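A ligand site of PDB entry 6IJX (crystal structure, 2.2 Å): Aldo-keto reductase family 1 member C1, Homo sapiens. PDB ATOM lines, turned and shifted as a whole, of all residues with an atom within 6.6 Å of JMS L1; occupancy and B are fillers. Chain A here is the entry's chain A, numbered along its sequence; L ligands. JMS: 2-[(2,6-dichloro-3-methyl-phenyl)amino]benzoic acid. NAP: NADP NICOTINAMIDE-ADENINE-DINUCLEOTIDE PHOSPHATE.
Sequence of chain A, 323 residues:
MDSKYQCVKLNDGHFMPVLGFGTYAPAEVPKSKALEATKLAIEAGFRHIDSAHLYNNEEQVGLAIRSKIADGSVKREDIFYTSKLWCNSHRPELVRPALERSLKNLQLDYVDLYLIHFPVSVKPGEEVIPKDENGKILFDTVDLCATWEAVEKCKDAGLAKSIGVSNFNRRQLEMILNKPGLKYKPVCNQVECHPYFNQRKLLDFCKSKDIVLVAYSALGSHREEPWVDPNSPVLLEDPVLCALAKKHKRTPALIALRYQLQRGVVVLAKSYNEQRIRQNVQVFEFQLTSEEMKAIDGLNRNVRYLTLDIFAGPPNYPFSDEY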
ATOM      1  N   TYR A  24     -18.135  28.705 -12.159  1.00  0.00           N
ATOM      2  CA  TYR A  24     -17.403  27.549 -11.659  1.00  0.00           C
ATOM      3  C   TYR A  24     -16.977  26.650 -12.816  1.00  0.00           C
ATOM      4  O   TYR A  24     -17.722  26.429 -13.774  1.00  0.00           O
ATOM      5  CB  TYR A  24     -18.233  26.713 -10.673  1.00  0.00           C
ATOM      6  CG  TYR A  24     -17.579  25.363 -10.444  1.00  0.00           C
ATOM      7  CD1 TYR A  24     -17.937  24.263 -11.215  1.00  0.00           C
ATOM      8  CD2 TYR A  24     -16.558  25.202  -9.516  1.00  0.00           C
ATOM      9  CE1 TYR A  24     -17.323  23.019 -11.052  1.00  0.00           C
ATOM     10  CE2 TYR A  24     -15.932  23.964  -9.341  1.00  0.00           C
ATOM     11  CZ  TYR A  24     -16.330  22.869 -10.109  1.00  0.00           C
ATOM     12  OH  TYR A  24     -15.726  21.633  -9.975  1.00  0.00           O
ATOM     13  N   ASP A  50     -22.372  34.746 -11.182  1.00  0.00           N
ATOM     14  CA  ASP A  50     -22.429  33.859 -10.037  1.00  0.00           C
ATOM     15  C   ASP A  50     -21.047  33.277  -9.736  1.00  0.00           C
ATOM     16  O   ASP A  50     -20.455  32.598 -10.578  1.00  0.00           O
ATOM     17  CB  ASP A  50     -23.426  32.728 -10.281  1.00  0.00           C
ATOM     18  CG  ASP A  50     -23.618  31.843  -9.049  1.00  0.00           C
ATOM     19  OD1 ASP A  50     -24.411  32.241  -8.156  1.00  0.00           O
ATOM     20  OD2 ASP A  50     -22.970  30.791  -8.974  1.00  0.00           O
ATOM     21  N   ALA A  52     -18.297  32.315  -5.986  1.00  0.00           N
ATOM     22  CA  ALA A  52     -18.263  31.854  -4.596  1.00  0.00           C
ATOM     23  C   ALA A  52     -16.819  31.738  -4.112  1.00  0.00           C
ATOM     24  O   ALA A  52     -15.913  31.521  -4.923  1.00  0.00           O
ATOM     25  CB  ALA A  52     -18.982  30.513  -4.457  1.00  0.00           C
ATOM     26  N   LEU A  54     -15.666  29.203  -2.703  1.00  0.00           N
ATOM     27  CA  LEU A  54     -15.265  27.846  -3.055  1.00  0.00           C
ATOM     28  C   LEU A  54     -14.565  27.781  -4.410  1.00  0.00           C
ATOM     29  O   LEU A  54     -13.641  26.996  -4.598  1.00  0.00           O
ATOM     30  CB  LEU A  54     -16.478  26.923  -3.057  1.00  0.00           C
ATOM     31  CG  LEU A  54     -16.205  25.450  -3.402  1.00  0.00           C
ATOM     32  CD1 LEU A  54     -15.265  24.782  -2.388  1.00  0.00           C
ATOM     33  CD2 LEU A  54     -17.511  24.694  -3.516  1.00  0.00           C
ATOM     34  N   TYR A  55     -15.013  28.594  -5.372  1.00  0.00           N
ATOM     35  CA  TYR A  55     -14.582  28.434  -6.752  1.00  0.00           C
ATOM     36  C   TYR A  55     -13.142  28.886  -6.985  1.00  0.00           C
ATOM     37  O   TYR A  55     -12.581  28.564  -8.037  1.00  0.00           O
ATOM     38  CB  TYR A  55     -15.513  29.197  -7.692  1.00  0.00           C
ATOM     39  CG  TYR A  55     -16.972  28.766  -7.619  1.00  0.00           C
ATOM     40  CD1 TYR A  55     -17.338  27.554  -7.037  1.00  0.00           C
ATOM     41  CD2 TYR A  55     -17.967  29.582  -8.122  1.00  0.00           C
ATOM     42  CE1 TYR A  55     -18.675  27.183  -6.953  1.00  0.00           C
ATOM     43  CE2 TYR A  55     -19.284  29.224  -8.066  1.00  0.00           C
ATOM     44  CZ  TYR A  55     -19.648  28.021  -7.482  1.00  0.00           C
ATOM     45  OH  TYR A  55     -20.975  27.666  -7.425  1.00  0.00           O
ATOM     46  N   LYS A  84     -20.637  33.482  -2.214  1.00  0.00           N
ATOM     47  CA  LYS A  84     -21.202  32.485  -1.307  1.00  0.00           C
ATOM     48  C   LYS A  84     -20.214  32.217  -0.166  1.00  0.00           C
ATOM     49  O   LYS A  84     -19.003  32.139  -0.376  1.00  0.00           O
ATOM     50  CB  LYS A  84     -21.527  31.184  -2.045  1.00  0.00           C
ATOM     51  CG  LYS A  84     -22.108  31.390  -3.470  1.00  0.00           C
ATOM     52  CD  LYS A  84     -22.942  30.159  -3.929  1.00  0.00           C
ATOM     53  CE  LYS A  84     -23.387  30.210  -5.407  1.00  0.00           C
ATOM     54  NZ  LYS A  84     -22.235  30.144  -6.374  1.00  0.00           N
ATOM     55  N   TRP A  86     -18.584  29.734   2.352  1.00  0.00           N
ATOM     56  CA  TRP A  86     -18.368  28.298   2.286  1.00  0.00           C
ATOM     57  C   TRP A  86     -18.523  27.664   3.660  1.00  0.00           C
ATOM     58  O   TRP A  86     -18.605  28.348   4.693  1.00  0.00           O
ATOM     59  CB  TRP A  86     -16.997  27.973   1.692  1.00  0.00           C
ATOM     60  CG  TRP A  86     -16.822  26.500   1.545  1.00  0.00           C
ATOM     61  CD1 TRP A  86     -15.865  25.733   2.133  1.00  0.00           C
ATOM     62  CD2 TRP A  86     -17.693  25.607   0.829  1.00  0.00           C
ATOM     63  NE1 TRP A  86     -16.055  24.408   1.796  1.00  0.00           N
ATOM     64  CE2 TRP A  86     -17.178  24.304   1.002  1.00  0.00           C
ATOM     65  CE3 TRP A  86     -18.844  25.772   0.060  1.00  0.00           C
ATOM     66  CZ2 TRP A  86     -17.769  23.185   0.429  1.00  0.00           C
ATOM     67  CZ3 TRP A  86     -19.434  24.663  -0.510  1.00  0.00           C
ATOM     68  CH2 TRP A  86     -18.893  23.381  -0.313  1.00  0.00           C
ATOM     69  N   CYS A  87     -18.570  26.335   3.678  1.00  0.00           N
ATOM     70  CA  CYS A  87     -18.896  25.582   4.885  1.00  0.00           C
ATOM     71  C   CYS A  87     -17.872  25.759   6.009  1.00  0.00           C
ATOM     72  O   CYS A  87     -18.186  25.513   7.174  1.00  0.00           O
ATOM     73  CB  CYS A  87     -19.059  24.112   4.523  1.00  0.00           C
ATOM     74  SG  CYS A  87     -20.295  23.836   3.175  1.00  0.00           S
ATOM     75  N   HIS A 117     -23.764  28.701   1.157  1.00  0.00           N
ATOM     76  CA  HIS A 117     -23.520  27.881  -0.028  1.00  0.00           C
ATOM     77  C   HIS A 117     -24.145  26.499   0.088  1.00  0.00           C
ATOM     78  O   HIS A 117     -24.713  25.981  -0.885  1.00  0.00           O
ATOM     79  CB  HIS A 117     -22.009  27.768  -0.214  1.00  0.00           C
ATOM     80  CG  HIS A 117     -21.570  27.389  -1.596  1.00  0.00           C
ATOM     81  ND1 HIS A 117     -20.393  27.845  -2.149  1.00  0.00           N
ATOM     82  CD2 HIS A 117     -22.128  26.576  -2.518  1.00  0.00           C
ATOM     83  CE1 HIS A 117     -20.247  27.326  -3.350  1.00  0.00           C
ATOM     84  NE2 HIS A 117     -21.283  26.547  -3.600  1.00  0.00           N
ATOM     85  N   PHE A 118     -24.046  25.888   1.275  1.00  0.00           N
ATOM     86  CA  PHE A 118     -24.448  24.507   1.539  1.00  0.00           C
ATOM     87  C   PHE A 118     -24.650  24.394   3.031  1.00  0.00           C
ATOM     88  O   PHE A 118     -23.798  24.876   3.781  1.00  0.00           O
ATOM     89  CB  PHE A 118     -23.369  23.535   1.064  1.00  0.00           C
ATOM     90  CG  PHE A 118     -23.835  22.098   0.956  1.00  0.00           C
ATOM     91  CD1 PHE A 118     -24.523  21.654  -0.160  1.00  0.00           C
ATOM     92  CD2 PHE A 118     -23.542  21.178   1.949  1.00  0.00           C
ATOM     93  CE1 PHE A 118     -24.930  20.340  -0.261  1.00  0.00           C
ATOM     94  CE2 PHE A 118     -23.940  19.852   1.845  1.00  0.00           C
ATOM     95  CZ  PHE A 118     -24.632  19.447   0.749  1.00  0.00           C
ATOM     96  N   VAL A 128     -10.916  23.936   2.432  1.00  0.00           N
ATOM     97  CA  VAL A 128     -12.351  24.006   2.174  1.00  0.00           C
ATOM     98  C   VAL A 128     -13.007  22.650   2.379  1.00  0.00           C
ATOM     99  O   VAL A 128     -14.190  22.574   2.736  1.00  0.00           O
ATOM    100  CB  VAL A 128     -12.637  24.558   0.751  1.00  0.00           C
ATOM    101  CG1 VAL A 128     -12.277  26.053   0.650  1.00  0.00           C
ATOM    102  CG2 VAL A 128     -11.899  23.732  -0.316  1.00  0.00           C
ATOM    103  N   ILE A 129     -12.249  21.566   2.206  1.00  0.00           N
ATOM    104  CA  ILE A 129     -12.731  20.206   2.436  1.00  0.00           C
ATOM    105  C   ILE A 129     -11.782  19.490   3.387  1.00  0.00           C
ATOM    106  O   ILE A 129     -10.996  18.641   2.951  1.00  0.00           O
ATOM    107  CB  ILE A 129     -12.875  19.429   1.120  1.00  0.00           C
ATOM    108  CG1 ILE A 129     -13.933  20.065   0.235  1.00  0.00           C
ATOM    109  CG2 ILE A 129     -13.272  18.018   1.376  1.00  0.00           C
ATOM    110  CD1 ILE A 129     -13.668  19.852  -1.245  1.00  0.00           C
ATOM    111  N   SER A 166     -28.486  28.448  -0.399  1.00  0.00           N
ATOM    112  CA  SER A 166     -28.275  27.513  -1.517  1.00  0.00           C
ATOM    113  C   SER A 166     -28.289  26.096  -0.976  1.00  0.00           C
ATOM    114  O   SER A 166     -27.766  25.855   0.113  1.00  0.00           O
ATOM    115  CB  SER A 166     -26.954  27.787  -2.232  1.00  0.00           C
ATOM    116  OG  SER A 166     -26.870  27.063  -3.450  1.00  0.00           O
ATOM    117  N   ASN A 167     -28.864  25.177  -1.748  1.00  0.00           N
ATOM    118  CA  ASN A 167     -28.938  23.767  -1.367  1.00  0.00           C
ATOM    119  C   ASN A 167     -29.659  23.569  -0.034  1.00  0.00           C
ATOM    120  O   ASN A 167     -29.300  22.708   0.755  1.00  0.00           O
ATOM    121  CB  ASN A 167     -27.539  23.135  -1.305  1.00  0.00           C
ATOM    122  CG  ASN A 167     -26.755  23.276  -2.623  1.00  0.00           C
ATOM    123  OD1 ASN A 167     -25.725  23.956  -2.695  1.00  0.00           O
ATOM    124  ND2 ASN A 167     -27.256  22.630  -3.671  1.00  0.00           N
ATOM    125  N   GLN A 190     -30.683  28.840  -4.149  1.00  0.00           N
ATOM    126  CA  GLN A 190     -30.048  28.426  -5.391  1.00  0.00           C
ATOM    127  C   GLN A 190     -29.815  26.918  -5.342  1.00  0.00           C
ATOM    128  O   GLN A 190     -29.070  26.432  -4.474  1.00  0.00           O
ATOM    129  CB  GLN A 190     -28.736  29.169  -5.621  1.00  0.00           C
ATOM    130  CG  GLN A 190     -28.129  28.895  -6.993  1.00  0.00           C
ATOM    131  CD  GLN A 190     -26.694  29.395  -7.121  1.00  0.00           C
ATOM    132  OE1 GLN A 190     -25.761  28.609  -7.309  1.00  0.00           O
ATOM    133  NE2 GLN A 190     -26.521  30.710  -7.033  1.00  0.00           N
ATOM    134  N   TYR A 216     -29.198  25.959 -10.803  1.00  0.00           N
ATOM    135  CA  TYR A 216     -27.854  25.654 -11.247  1.00  0.00           C
ATOM    136  C   TYR A 216     -27.830  24.292 -11.928  1.00  0.00           C
ATOM    137  O   TYR A 216     -28.773  23.493 -11.805  1.00  0.00           O
ATOM    138  CB  TYR A 216     -26.839  25.762 -10.088  1.00  0.00           C
ATOM    139  CG  TYR A 216     -26.770  24.664  -9.018  1.00  0.00           C
ATOM    140  CD1 TYR A 216     -26.441  23.354  -9.346  1.00  0.00           C
ATOM    141  CD2 TYR A 216     -26.936  24.985  -7.669  1.00  0.00           C
ATOM    142  CE1 TYR A 216     -26.328  22.383  -8.360  1.00  0.00           C
ATOM    143  CE2 TYR A 216     -26.832  24.024  -6.680  1.00  0.00           C
ATOM    144  CZ  TYR A 216     -26.513  22.721  -7.027  1.00  0.00           C
ATOM    145  OH  TYR A 216     -26.410  21.751  -6.040  1.00  0.00           O
ATOM    146  N   HIS A 222     -21.570  20.300 -15.444  1.00  0.00           N
ATOM    147  CA  HIS A 222     -20.253  20.008 -16.008  1.00  0.00           C
ATOM    148  C   HIS A 222     -20.034  18.530 -16.250  1.00  0.00           C
ATOM    149  O   HIS A 222     -19.191  18.169 -17.073  1.00  0.00           O
ATOM    150  CB  HIS A 222     -19.198  20.529 -15.038  1.00  0.00           C
ATOM    151  CG  HIS A 222     -19.655  20.492 -13.602  1.00  0.00           C
ATOM    152  ND1 HIS A 222     -19.637  19.331 -12.845  1.00  0.00           N
ATOM    153  CD2 HIS A 222     -20.166  21.458 -12.796  1.00  0.00           C
ATOM    154  CE1 HIS A 222     -20.082  19.606 -11.632  1.00  0.00           C
ATOM    155  NE2 HIS A 222     -20.413  20.887 -11.579  1.00  0.00           N
ATOM    156  N   GLU A 224     -18.524  16.634 -14.408  1.00  0.00           N
ATOM    157  CA  GLU A 224     -17.163  16.386 -13.964  1.00  0.00           C
ATOM    158  C   GLU A 224     -17.153  15.256 -12.941  1.00  0.00           C
ATOM    159  O   GLU A 224     -17.822  15.339 -11.903  1.00  0.00           O
ATOM    160  CB  GLU A 224     -16.576  17.680 -13.379  1.00  0.00           C
ATOM    161  CG  GLU A 224     -15.447  17.517 -12.341  1.00  0.00           C
ATOM    162  CD  GLU A 224     -15.030  18.847 -11.660  1.00  0.00           C
ATOM    163  OE1 GLU A 224     -13.891  18.911 -11.144  1.00  0.00           O
ATOM    164  OE2 GLU A 224     -15.834  19.812 -11.608  1.00  0.00           O
ATOM    165  N   TRP A 227     -17.805  14.209  -9.264  1.00  0.00           N
ATOM    166  CA  TRP A 227     -19.003  14.829  -8.717  1.00  0.00           C
ATOM    167  C   TRP A 227     -20.279  14.307  -9.351  1.00  0.00           C
ATOM    168  O   TRP A 227     -21.330  14.306  -8.701  1.00  0.00           O
ATOM    169  CB  TRP A 227     -18.919  16.342  -8.877  1.00  0.00           C
ATOM    170  CG  TRP A 227     -17.675  16.872  -8.292  1.00  0.00           C
ATOM    171  CD1 TRP A 227     -16.557  17.262  -8.962  1.00  0.00           C
ATOM    172  CD2 TRP A 227     -17.387  17.023  -6.895  1.00  0.00           C
ATOM    173  NE1 TRP A 227     -15.593  17.680  -8.066  1.00  0.00           N
ATOM    174  CE2 TRP A 227     -16.078  17.533  -6.800  1.00  0.00           C
ATOM    175  CE3 TRP A 227     -18.114  16.792  -5.724  1.00  0.00           C
ATOM    176  CZ2 TRP A 227     -15.478  17.819  -5.575  1.00  0.00           C
ATOM    177  CZ3 TRP A 227     -17.517  17.061  -4.514  1.00  0.00           C
ATOM    178  CH2 TRP A 227     -16.210  17.566  -4.441  1.00  0.00           C
ATOM    179  N   LEU A 306     -25.906  16.402  -8.940  1.00  0.00           N
ATOM    180  CA  LEU A 306     -24.962  16.832  -7.906  1.00  0.00           C
ATOM    181  C   LEU A 306     -25.514  16.404  -6.552  1.00  0.00           C
ATOM    182  O   LEU A 306     -26.152  17.176  -5.851  1.00  0.00           O
ATOM    183  CB  LEU A 306     -24.730  18.342  -7.979  1.00  0.00           C
ATOM    184  CG  LEU A 306     -23.462  18.767  -7.235  1.00  0.00           C
ATOM    185  CD1 LEU A 306     -22.226  18.195  -7.926  1.00  0.00           C
ATOM    186  CD2 LEU A 306     -23.368  20.280  -7.097  1.00  0.00           C
ATOM    187  N   LEU A 308     -23.658  15.402  -3.979  1.00  0.00           N
ATOM    188  CA  LEU A 308     -22.748  15.801  -2.922  1.00  0.00           C
ATOM    189  C   LEU A 308     -22.742  14.786  -1.768  1.00  0.00           C
ATOM    190  O   LEU A 308     -22.731  15.152  -0.599  1.00  0.00           O
ATOM    191  CB  LEU A 308     -23.083  17.197  -2.429  1.00  0.00           C
ATOM    192  CG  LEU A 308     -23.225  18.182  -3.585  1.00  0.00           C
ATOM    193  CD1 LEU A 308     -24.010  19.415  -3.231  1.00  0.00           C
ATOM    194  CD2 LEU A 308     -21.851  18.565  -4.049  1.00  0.00           C
ATOM    195  N   ILE A 310     -20.420  13.412  -0.628  1.00  0.00           N
ATOM    196  CA  ILE A 310     -19.243  13.731   0.186  1.00  0.00           C
ATOM    197  C   ILE A 310     -19.655  14.300   1.541  1.00  0.00           C
ATOM    198  O   ILE A 310     -18.960  14.103   2.543  1.00  0.00           O
ATOM    199  CB  ILE A 310     -18.331  14.695  -0.606  1.00  0.00           C
ATOM    200  CG1 ILE A 310     -16.972  14.870   0.075  1.00  0.00           C
ATOM    201  CG2 ILE A 310     -19.013  16.042  -0.804  1.00  0.00           C
ATOM    202  CD1 ILE A 310     -16.002  15.702  -0.772  1.00  0.00           C
ATOM    203  N   PHE A 311     -20.797  14.974   1.606  1.00  0.00           N
ATOM    204  CA  PHE A 311     -21.235  15.630   2.828  1.00  0.00           C
ATOM    205  C   PHE A 311     -22.457  14.978   3.448  1.00  0.00           C
ATOM    206  O   PHE A 311     -23.109  15.592   4.296  1.00  0.00           O
ATOM    207  CB  PHE A 311     -21.526  17.114   2.569  1.00  0.00           C
ATOM    208  CG  PHE A 311     -20.289  17.990   2.580  1.00  0.00           C
ATOM    209  CD1 PHE A 311     -19.014  17.427   2.611  1.00  0.00           C
ATOM    210  CD2 PHE A 311     -20.407  19.375   2.570  1.00  0.00           C
ATOM    211  CE1 PHE A 311     -17.880  18.227   2.616  1.00  0.00           C
ATOM    212  CE2 PHE A 311     -19.283  20.177   2.576  1.00  0.00           C
ATOM    213  CZ  PHE A 311     -18.009  19.609   2.585  1.00  0.00           C
HETATM  214  OXT JMS L   1     -20.776  24.620  -5.658  1.00  0.00           O
HETATM  215  C7  JMS L   1     -20.360  24.348  -6.859  1.00  0.00           C
HETATM  216  OH  JMS L   1     -20.499  25.123  -7.789  1.00  0.00           O
HETATM  217  C1  JMS L   1     -19.755  22.989  -7.043  1.00  0.00           C
HETATM  218  C6  JMS L   1     -19.513  22.550  -8.341  1.00  0.00           C
HETATM  219  C5  JMS L   1     -19.169  21.225  -8.570  1.00  0.00           C
HETATM  220  C4  JMS L   1     -19.071  20.337  -7.532  1.00  0.00           C
HETATM  221  C3  JMS L   1     -19.295  20.762  -6.228  1.00  0.00           C
HETATM  222  C2  JMS L   1     -19.626  22.088  -5.968  1.00  0.00           C
HETATM  223  N   JMS L   1     -19.733  22.554  -4.658  1.00  0.00           N
HETATM  224  C1B JMS L   1     -19.716  21.744  -3.496  1.00  0.00           C
HETATM  225  C2B JMS L   1     -18.620  20.968  -3.100  1.00  0.00           C
HETATM  226 CL1  JMS L   1     -17.163  21.032  -4.034  1.00  0.00          CL
HETATM  227  C3B JMS L   1     -18.624  20.166  -1.956  1.00  0.00           C
HETATM  228  C7B JMS L   1     -17.465  19.280  -1.578  1.00  0.00           C
HETATM  229  C4B JMS L   1     -19.763  20.188  -1.165  1.00  0.00           C
HETATM  230  C5B JMS L   1     -20.848  20.948  -1.503  1.00  0.00           C
HETATM  231  C6B JMS L   1     -20.819  21.717  -2.656  1.00  0.00           C
HETATM  232 CL2  JMS L   1     -22.200  22.685  -3.048  1.00  0.00          CL
HETATM  233  PA  NAP L   2     -24.213  23.993 -16.434  1.00  0.00           P
HETATM  234  O1A NAP L   2     -24.559  25.446 -16.524  1.00  0.00           O
HETATM  235  O2A NAP L   2     -25.445  23.186 -16.078  1.00  0.00           O
HETATM  236  O5B NAP L   2     -23.576  23.360 -17.760  1.00  0.00           O
HETATM  237  C5B NAP L   2     -22.186  23.669 -17.974  1.00  0.00           C
HETATM  238  C4B NAP L   2     -21.677  22.732 -19.030  1.00  0.00           C
HETATM  239  O4B NAP L   2     -22.491  22.900 -20.221  1.00  0.00           O
HETATM  240  C3B NAP L   2     -20.236  22.941 -19.466  1.00  0.00           C
HETATM  241  O3B NAP L   2     -19.647  21.688 -19.819  1.00  0.00           O
HETATM  242  C2B NAP L   2     -20.391  23.814 -20.711  1.00  0.00           C
HETATM  243  O2B NAP L   2     -19.277  23.591 -21.602  1.00  0.00           O
HETATM  244  C1B NAP L   2     -21.689  23.327 -21.305  1.00  0.00           C
HETATM  245  N9A NAP L   2     -22.441  24.335 -22.087  1.00  0.00           N
HETATM  246  C8A NAP L   2     -22.690  25.628 -21.745  1.00  0.00           C
HETATM  247  N7A NAP L   2     -23.391  26.291 -22.644  1.00  0.00           N
HETATM  248  C5A NAP L   2     -23.620  25.335 -23.631  1.00  0.00           C
HETATM  249  C6A NAP L   2     -24.340  25.398 -24.840  1.00  0.00           C
HETATM  250  N6A NAP L   2     -24.986  26.482 -25.267  1.00  0.00           N
HETATM  251  N1A NAP L   2     -24.396  24.273 -25.585  1.00  0.00           N
HETATM  252  C2A NAP L   2     -23.772  23.168 -25.141  1.00  0.00           C
HETATM  253  N3A NAP L   2     -23.073  23.004 -24.018  1.00  0.00           N
HETATM  254  C4A NAP L   2     -23.029  24.129 -23.304  1.00  0.00           C
HETATM  255  O3  NAP L   2     -23.009  23.671 -15.437  1.00  0.00           O
HETATM  256  PN  NAP L   2     -22.733  24.100 -13.930  1.00  0.00           P
HETATM  257  O1N NAP L   2     -21.302  24.446 -13.756  1.00  0.00           O
HETATM  258  O2N NAP L   2     -23.353  23.089 -13.056  1.00  0.00           O
HETATM  259  O5D NAP L   2     -23.475  25.492 -14.054  1.00  0.00           O
HETATM  260  C5D NAP L   2     -24.234  26.124 -13.033  1.00  0.00           C
HETATM  261  C4D NAP L   2     -23.458  27.220 -12.359  1.00  0.00           C
HETATM  262  O4D NAP L   2     -24.154  27.498 -11.117  1.00  0.00           O
HETATM  263  C3D NAP L   2     -22.008  26.919 -11.971  1.00  0.00           C
HETATM  264  O3D NAP L   2     -21.029  27.373 -12.899  1.00  0.00           O
HETATM  265  C2D NAP L   2     -21.868  27.662 -10.642  1.00  0.00           C
HETATM  266  O2D NAP L   2     -21.773  29.086 -10.742  1.00  0.00           O
HETATM  267  C1D NAP L   2     -23.249  27.447 -10.045  1.00  0.00           C
HETATM  268  N1N NAP L   2     -23.446  26.151  -9.314  1.00  0.00           N
HETATM  269  C2N NAP L   2     -23.783  26.369  -8.026  1.00  0.00           C
HETATM  270  C3N NAP L   2     -23.851  25.315  -7.137  1.00  0.00           C
HETATM  271  C7N NAP L   2     -24.225  25.568  -5.705  1.00  0.00           C
HETATM  272  O7N NAP L   2     -24.617  26.715  -5.353  1.00  0.00           O
HETATM  273  N7N NAP L   2     -24.189  24.571  -4.908  1.00  0.00           N
HETATM  274  C4N NAP L   2     -23.619  24.035  -7.609  1.00  0.00           C
HETATM  275  C5N NAP L   2     -23.324  23.825  -8.945  1.00  0.00           C
HETATM  276  C6N NAP L   2     -23.238  24.906  -9.787  1.00  0.00           C
HETATM  277  P2B NAP L   2     -18.427  24.816 -22.092  1.00  0.00           P
HETATM  278  O1X NAP L   2     -17.911  25.575 -20.914  1.00  0.00           O
HETATM  279  O2X NAP L   2     -17.340  24.208 -22.962  1.00  0.00           O
HETATM  280  O3X NAP L   2     -19.377  25.630 -22.967  1.00  0.00           O
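OH of Tyr 55 lies within hydrogen-bond range of NZ of Lys 84, at 3.0 Å. The backbone carbonyl oxygen (O) of His 117 lies close to the side-chain amide oxygen (OD1) of Asn 167. ND1 of His 222 lies close to N of Glu 224 (3.3 Å). The side-chain hydroxyl (OH) of Tyr 24 is in hydrogen-bond range of the side-chain carboxylate (OE2) of Glu 224, 2.4 Å away. The side-chain hydroxyl of Tyr 216 sits at hydrogen-bond distance from the side-chain amide nitrogen of Asn 167. N of Asn 167 is in hydrogen-bond range of O of Gln 190 (3.0 Å). The side-chain amide oxygen (OD1) of Asn 167 sits at hydrogen-bond distance from the side-chain hydroxyl (OG) of Ser 166 (3.4 Å). O of Phe 118 sits at hydrogen-bond distance from SG of Cys 87.
Residues that only touch JMS L1: Tyr 24 (3.5 Å), Leu 54 (3.3 Å), Trp 86 (3.3 Å), Phe 118 (3.8 Å), Ile 129 (3.9 Å), Asn 167 (3.8 Å), His 222 (3.3 Å), Trp 227 (3.6 Å), Leu 306 (3.8 Å), Leu 308 (3.6 Å), Ile 310 (3.7 Å) and Phe 311 (3.8 Å). Hydrophobic or aromatic side chains that line JMS L1: Tyr 24, Leu 54, Tyr 55, Trp 86, His 117, Phe 118, Ile 129, His 222, Trp 227, Leu 306, Leu 308, Ile 310 and Phe 311. 14 residues have an atom within 4 Å of JMS L1: Tyr 24, Leu 54, Tyr 55, Trp 86, His 117, Phe 118, Ile 129, Asn 167, His 222, Trp 227, Leu 306, Leu 308, Ile 310 and Phe 311.
An oxygen (OH) of JMS L1 sits at hydrogen-bond distance from the side-chain hydroxyl (OH) of Tyr 55, at 2.6 Å. An oxygen (OXT) of JMS L1 is in hydrogen-bond range of a ring nitrogen (NE2) of His 117, 2.9 Å away. An oxygen (O3D) of NAP L2 is in hydrogen-bond range of the backbone NH (N) of Tyr 24 (3.3 Å). The side-chain amide oxygen (OD1) of Asn 167 lies within hydrogen-bond range of a nitrogen (N7N) of NAP L2 (2.8 Å). An oxygen (O2D) of NAP L2 is in hydrogen-bond range of the side-chain carboxylate (OD2) of Asp 50. The side-chain amide oxygen (OE1) of Gln 190 lies close to an oxygen (O7N) of NAP L2 (3.0 Å). The side-chain hydroxyl (OG) of Ser 166 lies within hydrogen-bond range of an oxygen (O7N) of NAP L2 (3.0 Å).
A nitrogen (N7N) of NAP L2 sits close to an oxygen (OXT) of JMS L1 (3.5 Å).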
